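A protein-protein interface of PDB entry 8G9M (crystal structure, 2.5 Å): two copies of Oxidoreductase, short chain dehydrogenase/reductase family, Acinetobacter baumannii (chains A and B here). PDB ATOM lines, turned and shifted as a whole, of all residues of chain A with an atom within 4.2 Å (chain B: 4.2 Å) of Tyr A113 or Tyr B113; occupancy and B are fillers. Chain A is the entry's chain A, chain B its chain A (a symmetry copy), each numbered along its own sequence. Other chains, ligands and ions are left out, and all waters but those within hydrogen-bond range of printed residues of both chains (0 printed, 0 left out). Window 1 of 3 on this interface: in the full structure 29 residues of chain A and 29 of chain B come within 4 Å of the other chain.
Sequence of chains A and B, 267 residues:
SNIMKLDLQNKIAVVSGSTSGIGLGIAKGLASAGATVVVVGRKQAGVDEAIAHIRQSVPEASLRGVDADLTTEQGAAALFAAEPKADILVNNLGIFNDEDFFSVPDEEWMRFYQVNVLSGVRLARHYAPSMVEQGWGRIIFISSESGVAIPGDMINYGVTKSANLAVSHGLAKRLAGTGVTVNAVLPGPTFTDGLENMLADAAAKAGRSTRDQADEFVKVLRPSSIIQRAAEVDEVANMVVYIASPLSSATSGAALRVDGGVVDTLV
O of Tyr A113 lies within hydrogen-bond range of N of Leu A118 (3.1 Å). The backbone carbonyl oxygen (O) of Tyr B113 sits at hydrogen-bond distance from the backbone NH (N) of Leu B118, at 3.1 Å.
Trp A109 touches Tyr B113 (O to CE2, 3.7 Å). Met A110 touches Met B110. Met A110 touches Tyr B113. SD of Met A110 touches CB of Gln B114 (3.7 Å). Tyr A113 touches Trp B109 (CE2 to O, 3.7 Å). Tyr A113 touches Met B110 (CD2 to SD, 3.98 Å). Tyr A113 touches Tyr B113 (CD1 to CD1, 3.4 Å). Tyr A113 touches Val B159. Met B110 touches Gln A114 (SD to CB, 3.7 Å). OH of Tyr B113 touches CG1 of Val A159 (3.6 Å).
Of the printed residues of chain B, Tyr A113 touches Trp B109, Met B110, Tyr B113 and Val B159. Of the printed residues of chain B, Gln A114 touches Met B110 (3.7 Å). Tyr B113 touches just these residues of chain A: Trp A109 (3.7 Å), Met A110 (3.98 Å), Tyr A113 (3.4 Å) and Val A159 (3.6 Å). Asn B116 touches none of the printed residues of chain A. Of the printed residues of chain A, Leu B118 touches Trp A109 (3.6 Å). The nearest residue of chain B that does not touch Tyr A113 is Asn B156 (4.1 Å). The nearest residue of chain A that does not touch Tyr B113 is Asn A156 (4.1 Å).
Of the 12 printed residues of chain B, 6 touch a printed residue of chain A. Hydrophobic or aromatic side chains of chain B within 4 Å of the printed part of chain A: Trp B109, Met B110, Tyr B113, Leu B118 and Val B159. Of the 12 printed residues of chain A, 6 touch a printed residue of chain B. Printed residues of chain A that touch a printed residue of chain B: Trp A109, Met A110, Tyr A113, Gln A114, Leu A118 and Val A159. Hydrophobic or aromatic side chains of chain A that line the printed part of chain B: Trp A109, Met A110, Tyr A113, Leu A118 and Val A159. Among the printed residues, no Asp or Glu carboxylate lies within 4 Å of a Lys or Arg side-chain nitrogen of the other chain.
Trp A109 touches Leu B118, and with the chains exchanged Leu A118 touches Trp B109. Met A110 touches its own counterpart, Met B110. Tyr B113 touches its own counterpart, Tyr A113. Tyr A113 touches Val B159, and with the chains exchanged Val A159 touches Tyr B113. Positions printed for both chains: 109, 110, 111, 112, 113, 114, 115, 116, 117, 118, 156 and 159.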
ATOM      1  N   TRP A 109     -13.256  -8.661  17.298  1.00  0.00           N
ATOM      2  CA  TRP A 109     -13.149  -8.222  15.909  1.00  0.00           C
ATOM      3  C   TRP A 109     -12.607  -9.344  15.032  1.00  0.00           C
ATOM      4  O   TRP A 109     -13.174  -9.662  13.977  1.00  0.00           O
ATOM      5  CB  TRP A 109     -12.250  -6.985  15.815  1.00  0.00           C
ATOM      6  CG  TRP A 109     -12.879  -5.715  16.326  1.00  0.00           C
ATOM      7  CD1 TRP A 109     -12.795  -5.208  17.591  1.00  0.00           C
ATOM      8  CD2 TRP A 109     -13.681  -4.791  15.579  1.00  0.00           C
ATOM      9  NE1 TRP A 109     -13.499  -4.031  17.680  1.00  0.00           N
ATOM     10  CE2 TRP A 109     -14.051  -3.753  16.457  1.00  0.00           C
ATOM     11  CE3 TRP A 109     -14.123  -4.742  14.254  1.00  0.00           C
ATOM     12  CZ2 TRP A 109     -14.843  -2.680  16.054  1.00  0.00           C
ATOM     13  CZ3 TRP A 109     -14.908  -3.677  13.855  1.00  0.00           C
ATOM     14  CH2 TRP A 109     -15.261  -2.660  14.752  1.00  0.00           C
ATOM     15  N   MET A 110     -11.510  -9.970  15.471  1.00  0.00           N
ATOM     16  CA  MET A 110     -10.905 -11.044  14.690  1.00  0.00           C
ATOM     17  C   MET A 110     -11.836 -12.247  14.580  1.00  0.00           C
ATOM     18  O   MET A 110     -11.909 -12.884  13.523  1.00  0.00           O
ATOM     19  CB  MET A 110      -9.569 -11.455  15.308  1.00  0.00           C
ATOM     20  CG  MET A 110      -8.521 -10.356  15.294  1.00  0.00           C
ATOM     21  SD  MET A 110      -7.781 -10.136  13.667  1.00  0.00           S
ATOM     22  CE  MET A 110      -6.675 -11.544  13.608  1.00  0.00           C
ATOM     23  N   ARG A 111     -12.561 -12.569  15.655  1.00  0.00           N
ATOM     24  CA  ARG A 111     -13.474 -13.705  15.618  1.00  0.00           C
ATOM     25  C   ARG A 111     -14.637 -13.446  14.673  1.00  0.00           C
ATOM     26  O   ARG A 111     -15.057 -14.346  13.939  1.00  0.00           O
ATOM     27  CB  ARG A 111     -13.988 -14.018  17.023  1.00  0.00           C
ATOM     28  CG  ARG A 111     -14.801 -15.302  17.107  1.00  0.00           C
ATOM     29  CD  ARG A 111     -15.227 -15.610  18.534  1.00  0.00           C
ATOM     30  NE  ARG A 111     -16.224 -14.666  19.029  1.00  0.00           N
ATOM     31  CZ  ARG A 111     -17.538 -14.843  18.924  1.00  0.00           C
ATOM     32  NH1 ARG A 111     -18.018 -15.931  18.336  1.00  0.00           N
ATOM     33  NH2 ARG A 111     -18.372 -13.932  19.405  1.00  0.00           N
ATOM     34  N   PHE A 112     -15.176 -12.224  14.681  1.00  0.00           N
ATOM     35  CA  PHE A 112     -16.241 -11.892  13.744  1.00  0.00           C
ATOM     36  C   PHE A 112     -15.744 -11.969  12.309  1.00  0.00           C
ATOM     37  O   PHE A 112     -16.458 -12.451  11.422  1.00  0.00           O
ATOM     38  CB  PHE A 112     -16.800 -10.504  14.050  1.00  0.00           C
ATOM     39  CG  PHE A 112     -18.049 -10.527  14.885  1.00  0.00           C
ATOM     40  CD1 PHE A 112     -18.036 -11.065  16.162  1.00  0.00           C
ATOM     41  CD2 PHE A 112     -19.238 -10.015  14.391  1.00  0.00           C
ATOM     42  CE1 PHE A 112     -19.186 -11.087  16.932  1.00  0.00           C
ATOM     43  CE2 PHE A 112     -20.390 -10.035  15.153  1.00  0.00           C
ATOM     44  CZ  PHE A 112     -20.365 -10.572  16.424  1.00  0.00           C
ATOM     45  N   TYR A 113     -14.514 -11.514  12.060  1.00  0.00           N
ATOM     46  CA  TYR A 113     -13.961 -11.626  10.713  1.00  0.00           C
ATOM     47  C   TYR A 113     -13.796 -13.083  10.300  1.00  0.00           C
ATOM     48  O   TYR A 113     -14.111 -13.455   9.164  1.00  0.00           O
ATOM     49  CB  TYR A 113     -12.623 -10.898  10.631  1.00  0.00           C
ATOM     50  CG  TYR A 113     -12.095 -10.723   9.225  1.00  0.00           C
ATOM     51  CD1 TYR A 113     -12.749  -9.905   8.312  1.00  0.00           C
ATOM     52  CD2 TYR A 113     -10.937 -11.368   8.810  1.00  0.00           C
ATOM     53  CE1 TYR A 113     -12.266  -9.736   7.025  1.00  0.00           C
ATOM     54  CE2 TYR A 113     -10.447 -11.208   7.526  1.00  0.00           C
ATOM     55  CZ  TYR A 113     -11.113 -10.388   6.638  1.00  0.00           C
ATOM     56  OH  TYR A 113     -10.630 -10.221   5.359  1.00  0.00           O
ATOM     57  N   GLN A 114     -13.302 -13.923  11.213  1.00  0.00           N
ATOM     58  CA  GLN A 114     -13.062 -15.325  10.886  1.00  0.00           C
ATOM     59  C   GLN A 114     -14.370 -16.080  10.672  1.00  0.00           C
ATOM     60  O   GLN A 114     -14.446 -16.970   9.818  1.00  0.00           O
ATOM     61  CB  GLN A 114     -12.237 -15.980  11.994  1.00  0.00           C
ATOM     62  CG  GLN A 114     -11.906 -17.446  11.767  1.00  0.00           C
ATOM     63  CD  GLN A 114     -11.460 -18.141  13.041  1.00  0.00           C
ATOM     64  OE1 GLN A 114     -12.276 -18.705  13.773  1.00  0.00           O
ATOM     65  NE2 GLN A 114     -10.162 -18.097  13.317  1.00  0.00           N
ATOM     66  N   VAL A 115     -15.408 -15.734  11.431  1.00  0.00           N
ATOM     67  CA  VAL A 115     -16.671 -16.460  11.350  1.00  0.00           C
ATOM     68  C   VAL A 115     -17.488 -15.996  10.152  1.00  0.00           C
ATOM     69  O   VAL A 115     -18.009 -16.813   9.383  1.00  0.00           O
ATOM     70  CB  VAL A 115     -17.456 -16.298  12.666  1.00  0.00           C
ATOM     71  CG1 VAL A 115     -18.935 -16.561  12.443  1.00  0.00           C
ATOM     72  CG2 VAL A 115     -16.899 -17.225  13.737  1.00  0.00           C
ATOM     73  N   ASN A 116     -17.604 -14.681   9.966  1.00  0.00           N
ATOM     74  CA  ASN A 116     -18.516 -14.122   8.974  1.00  0.00           C
ATOM     75  C   ASN A 116     -17.910 -14.010   7.583  1.00  0.00           C
ATOM     76  O   ASN A 116     -18.638 -14.133   6.591  1.00  0.00           O
ATOM     77  CB  ASN A 116     -18.993 -12.737   9.427  1.00  0.00           C
ATOM     78  CG  ASN A 116     -19.840 -12.794  10.685  1.00  0.00           C
ATOM     79  OD1 ASN A 116     -20.280 -13.864  11.105  1.00  0.00           O
ATOM     80  ND2 ASN A 116     -20.076 -11.634  11.290  1.00  0.00           N
ATOM     81  N   VAL A 117     -16.606 -13.776   7.477  1.00  0.00           N
ATOM     82  CA  VAL A 117     -15.951 -13.514   6.201  1.00  0.00           C
ATOM     83  C   VAL A 117     -15.101 -14.698   5.753  1.00  0.00           C
ATOM     84  O   VAL A 117     -15.236 -15.179   4.627  1.00  0.00           O
ATOM     85  CB  VAL A 117     -15.108 -12.220   6.265  1.00  0.00           C
ATOM     86  CG1 VAL A 117     -14.464 -11.936   4.916  1.00  0.00           C
ATOM     87  CG2 VAL A 117     -15.967 -11.044   6.705  1.00  0.00           C
ATOM     88  N   LEU A 118     -14.216 -15.185   6.627  1.00  0.00           N
ATOM     89  CA  LEU A 118     -13.249 -16.189   6.196  1.00  0.00           C
ATOM     90  C   LEU A 118     -13.903 -17.543   5.940  1.00  0.00           C
ATOM     91  O   LEU A 118     -13.374 -18.343   5.164  1.00  0.00           O
ATOM     92  CB  LEU A 118     -12.126 -16.322   7.223  1.00  0.00           C
ATOM     93  CG  LEU A 118     -10.964 -17.217   6.782  1.00  0.00           C
ATOM     94  CD1 LEU A 118     -10.243 -16.603   5.594  1.00  0.00           C
ATOM     95  CD2 LEU A 118     -10.001 -17.458   7.926  1.00  0.00           C
ATOM     96  N   ASN A 156     -19.045  -3.858  14.101  1.00  0.00           N
ATOM     97  CA  ASN A 156     -18.342  -5.085  13.727  1.00  0.00           C
ATOM     98  C   ASN A 156     -19.107  -5.849  12.649  1.00  0.00           C
ATOM     99  O   ASN A 156     -18.537  -6.255  11.625  1.00  0.00           O
ATOM    100  CB  ASN A 156     -18.137  -5.954  14.969  1.00  0.00           C
ATOM    101  CG  ASN A 156     -17.000  -6.949  14.813  1.00  0.00           C
ATOM    102  OD1 ASN A 156     -16.633  -7.639  15.764  1.00  0.00           O
ATOM    103  ND2 ASN A 156     -16.438  -7.029  13.611  1.00  0.00           N
ATOM    104  N   VAL A 159     -19.132  -4.062   9.284  1.00  0.00           N
ATOM    105  CA  VAL A 159     -17.812  -4.188   8.674  1.00  0.00           C
ATOM    106  C   VAL A 159     -17.672  -5.546   7.999  1.00  0.00           C
ATOM    107  O   VAL A 159     -17.194  -5.646   6.863  1.00  0.00           O
ATOM    108  CB  VAL A 159     -16.711  -3.961   9.724  1.00  0.00           C
ATOM    109  CG1 VAL A 159     -15.368  -4.461   9.208  1.00  0.00           C
ATOM    110  CG2 VAL A 159     -16.625  -2.491  10.084  1.00  0.00           C
ATOM    111  N   TRP B 109      -5.279 -13.982   5.332  1.00  0.00           N
ATOM    112  CA  TRP B 109      -6.491 -13.172   5.430  1.00  0.00           C
ATOM    113  C   TRP B 109      -6.603 -12.537   6.810  1.00  0.00           C
ATOM    114  O   TRP B 109      -6.827 -11.324   6.940  1.00  0.00           O
ATOM    115  CB  TRP B 109      -7.724 -14.032   5.133  1.00  0.00           C
ATOM    116  CG  TRP B 109      -7.900 -14.393   3.681  1.00  0.00           C
ATOM    117  CD1 TRP B 109      -7.440 -15.514   3.052  1.00  0.00           C
ATOM    118  CD2 TRP B 109      -8.591 -13.631   2.684  1.00  0.00           C
ATOM    119  NE1 TRP B 109      -7.796 -15.495   1.725  1.00  0.00           N
ATOM    120  CE2 TRP B 109      -8.504 -14.349   1.474  1.00  0.00           C
ATOM    121  CE3 TRP B 109      -9.273 -12.410   2.695  1.00  0.00           C
ATOM    122  CZ2 TRP B 109      -9.072 -13.887   0.289  1.00  0.00           C
ATOM    123  CZ3 TRP B 109      -9.836 -11.954   1.518  1.00  0.00           C
ATOM    124  CH2 TRP B 109      -9.732 -12.690   0.331  1.00  0.00           C
ATOM    125  N   MET B 110      -6.427 -13.348   7.859  1.00  0.00           N
ATOM    126  CA  MET B 110      -6.535 -12.835   9.220  1.00  0.00           C
ATOM    127  C   MET B 110      -5.440 -11.818   9.522  1.00  0.00           C
ATOM    128  O   MET B 110      -5.690 -10.815  10.201  1.00  0.00           O
ATOM    129  CB  MET B 110      -6.486 -13.988  10.222  1.00  0.00           C
ATOM    130  CG  MET B 110      -7.649 -14.958  10.101  1.00  0.00           C
ATOM    131  SD  MET B 110      -9.163 -14.304  10.824  1.00  0.00           S
ATOM    132  CE  MET B 110      -8.826 -14.524  12.569  1.00  0.00           C
ATOM    133  N   ARG B 111      -4.223 -12.050   9.022  1.00  0.00           N
ATOM    134  CA  ARG B 111      -3.131 -11.117   9.269  1.00  0.00           C
ATOM    135  C   ARG B 111      -3.374  -9.788   8.570  1.00  0.00           C
ATOM    136  O   ARG B 111      -3.098  -8.726   9.136  1.00  0.00           O
ATOM    137  CB  ARG B 111      -1.803 -11.723   8.815  1.00  0.00           C
ATOM    138  CG  ARG B 111      -0.586 -10.895   9.203  1.00  0.00           C
ATOM    139  CD  ARG B 111       0.713 -11.574   8.796  1.00  0.00           C
ATOM    140  NE  ARG B 111       0.895 -11.596   7.348  1.00  0.00           N
ATOM    141  CZ  ARG B 111       1.529 -10.652   6.660  1.00  0.00           C
ATOM    142  NH1 ARG B 111       2.043  -9.603   7.287  1.00  0.00           N
ATOM    143  NH2 ARG B 111       1.649 -10.757   5.343  1.00  0.00           N
ATOM    144  N   PHE B 112      -3.884  -9.826   7.337  1.00  0.00           N
ATOM    145  CA  PHE B 112      -4.212  -8.585   6.646  1.00  0.00           C
ATOM    146  C   PHE B 112      -5.309  -7.830   7.379  1.00  0.00           C
ATOM    147  O   PHE B 112      -5.257  -6.600   7.491  1.00  0.00           O
ATOM    148  CB  PHE B 112      -4.623  -8.876   5.204  1.00  0.00           C
ATOM    149  CG  PHE B 112      -3.510  -8.700   4.211  1.00  0.00           C
ATOM    150  CD1 PHE B 112      -2.363  -9.473   4.290  1.00  0.00           C
ATOM    151  CD2 PHE B 112      -3.609  -7.758   3.200  1.00  0.00           C
ATOM    152  CE1 PHE B 112      -1.337  -9.311   3.376  1.00  0.00           C
ATOM    153  CE2 PHE B 112      -2.588  -7.590   2.285  1.00  0.00           C
ATOM    154  CZ  PHE B 112      -1.451  -8.366   2.372  1.00  0.00           C
ATOM    155  N   TYR B 113      -6.305  -8.549   7.901  1.00  0.00           N
ATOM    156  CA  TYR B 113      -7.350  -7.882   8.673  1.00  0.00           C
ATOM    157  C   TYR B 113      -6.785  -7.249   9.939  1.00  0.00           C
ATOM    158  O   TYR B 113      -7.142  -6.118  10.290  1.00  0.00           O
ATOM    159  CB  TYR B 113      -8.457  -8.871   9.025  1.00  0.00           C
ATOM    160  CG  TYR B 113      -9.706  -8.231   9.588  1.00  0.00           C
ATOM    161  CD1 TYR B 113     -10.505  -7.409   8.803  1.00  0.00           C
ATOM    162  CD2 TYR B 113     -10.094  -8.456  10.903  1.00  0.00           C
ATOM    163  CE1 TYR B 113     -11.654  -6.826   9.313  1.00  0.00           C
ATOM    164  CE2 TYR B 113     -11.239  -7.877  11.422  1.00  0.00           C
ATOM    165  CZ  TYR B 113     -12.017  -7.065  10.622  1.00  0.00           C
ATOM    166  OH  TYR B 113     -13.159  -6.488  11.130  1.00  0.00           O
ATOM    167  N   GLN B 114      -5.901  -7.965  10.637  1.00  0.00           N
ATOM    168  CA  GLN B 114      -5.349  -7.457  11.889  1.00  0.00           C
ATOM    169  C   GLN B 114      -4.429  -6.264  11.650  1.00  0.00           C
ATOM    170  O   GLN B 114      -4.391  -5.331  12.460  1.00  0.00           O
ATOM    171  CB  GLN B 114      -4.604  -8.576  12.617  1.00  0.00           C
ATOM    172  CG  GLN B 114      -3.989  -8.177  13.949  1.00  0.00           C
ATOM    173  CD  GLN B 114      -2.941  -9.169  14.421  1.00  0.00           C
ATOM    174  OE1 GLN B 114      -1.754  -9.025  14.123  1.00  0.00           O
ATOM    175  NE2 GLN B 114      -3.377 -10.188  15.153  1.00  0.00           N
ATOM    176  N   VAL B 115      -3.689  -6.274  10.543  1.00  0.00           N
ATOM    177  CA  VAL B 115      -2.721  -5.215  10.279  1.00  0.00           C
ATOM    178  C   VAL B 115      -3.409  -3.978   9.717  1.00  0.00           C
ATOM    179  O   VAL B 115      -3.161  -2.853  10.167  1.00  0.00           O
ATOM    180  CB  VAL B 115      -1.622  -5.731   9.329  1.00  0.00           C
ATOM    181  CG1 VAL B 115      -0.936  -4.573   8.626  1.00  0.00           C
ATOM    182  CG2 VAL B 115      -0.611  -6.574  10.092  1.00  0.00           C
ATOM    183  N   ASN B 116      -4.292  -4.166   8.736  1.00  0.00           N
ATOM    184  CA  ASN B 116      -4.865  -3.049   7.993  1.00  0.00           C
ATOM    185  C   ASN B 116      -6.101  -2.449   8.648  1.00  0.00           C
ATOM    186  O   ASN B 116      -6.332  -1.242   8.518  1.00  0.00           O
ATOM    187  CB  ASN B 116      -5.218  -3.496   6.570  1.00  0.00           C
ATOM    188  CG  ASN B 116      -3.994  -3.866   5.753  1.00  0.00           C
ATOM    189  OD1 ASN B 116      -2.862  -3.576   6.142  1.00  0.00           O
ATOM    190  ND2 ASN B 116      -4.218  -4.505   4.610  1.00  0.00           N
ATOM    191  N   VAL B 117      -6.902  -3.252   9.342  1.00  0.00           N
ATOM    192  CA  VAL B 117      -8.178  -2.811   9.891  1.00  0.00           C
ATOM    193  C   VAL B 117      -8.114  -2.659  11.408  1.00  0.00           C
ATOM    194  O   VAL B 117      -8.478  -1.615  11.950  1.00  0.00           O
ATOM    195  CB  VAL B 117      -9.320  -3.768   9.479  1.00  0.00           C
ATOM    196  CG1 VAL B 117     -10.652  -3.274  10.023  1.00  0.00           C
ATOM    197  CG2 VAL B 117      -9.379  -3.907   7.965  1.00  0.00           C
ATOM    198  N   LEU B 118      -7.650  -3.696  12.110  1.00  0.00           N
ATOM    199  CA  LEU B 118      -7.740  -3.682  13.567  1.00  0.00           C
ATOM    200  C   LEU B 118      -6.769  -2.686  14.192  1.00  0.00           C
ATOM    201  O   LEU B 118      -7.010  -2.211  15.306  1.00  0.00           O
ATOM    202  CB  LEU B 118      -7.504  -5.084  14.127  1.00  0.00           C
ATOM    203  CG  LEU B 118      -7.756  -5.216  15.632  1.00  0.00           C
ATOM    204  CD1 LEU B 118      -9.225  -4.986  15.946  1.00  0.00           C
ATOM    205  CD2 LEU B 118      -7.306  -6.571  16.140  1.00  0.00           C
ATOM    206  N   ASN B 156      -7.702  -9.512  -1.067  1.00  0.00           N
ATOM    207  CA  ASN B 156      -7.497  -9.309   0.367  1.00  0.00           C
ATOM    208  C   ASN B 156      -7.370  -7.824   0.698  1.00  0.00           C
ATOM    209  O   ASN B 156      -8.033  -7.314   1.615  1.00  0.00           O
ATOM    210  CB  ASN B 156      -6.253 -10.076   0.819  1.00  0.00           C
ATOM    211  CG  ASN B 156      -6.249 -10.371   2.308  1.00  0.00           C
ATOM    212  OD1 ASN B 156      -5.376 -11.081   2.806  1.00  0.00           O
ATOM    213  ND2 ASN B 156      -7.224  -9.824   3.028  1.00  0.00           N
ATOM    214  N   VAL B 159     -10.628  -5.904   0.227  1.00  0.00           N
ATOM    215  CA  VAL B 159     -11.536  -6.243   1.318  1.00  0.00           C
ATOM    216  C   VAL B 159     -11.191  -5.435   2.561  1.00  0.00           C
ATOM    217  O   VAL B 159     -12.073  -4.877   3.224  1.00  0.00           O
ATOM    218  CB  VAL B 159     -11.500  -7.756   1.599  1.00  0.00           C
ATOM    219  CG1 VAL B 159     -12.126  -8.065   2.952  1.00  0.00           C
ATOM    220  CG2 VAL B 159     -12.219  -8.511   0.498  1.00  0.00           C
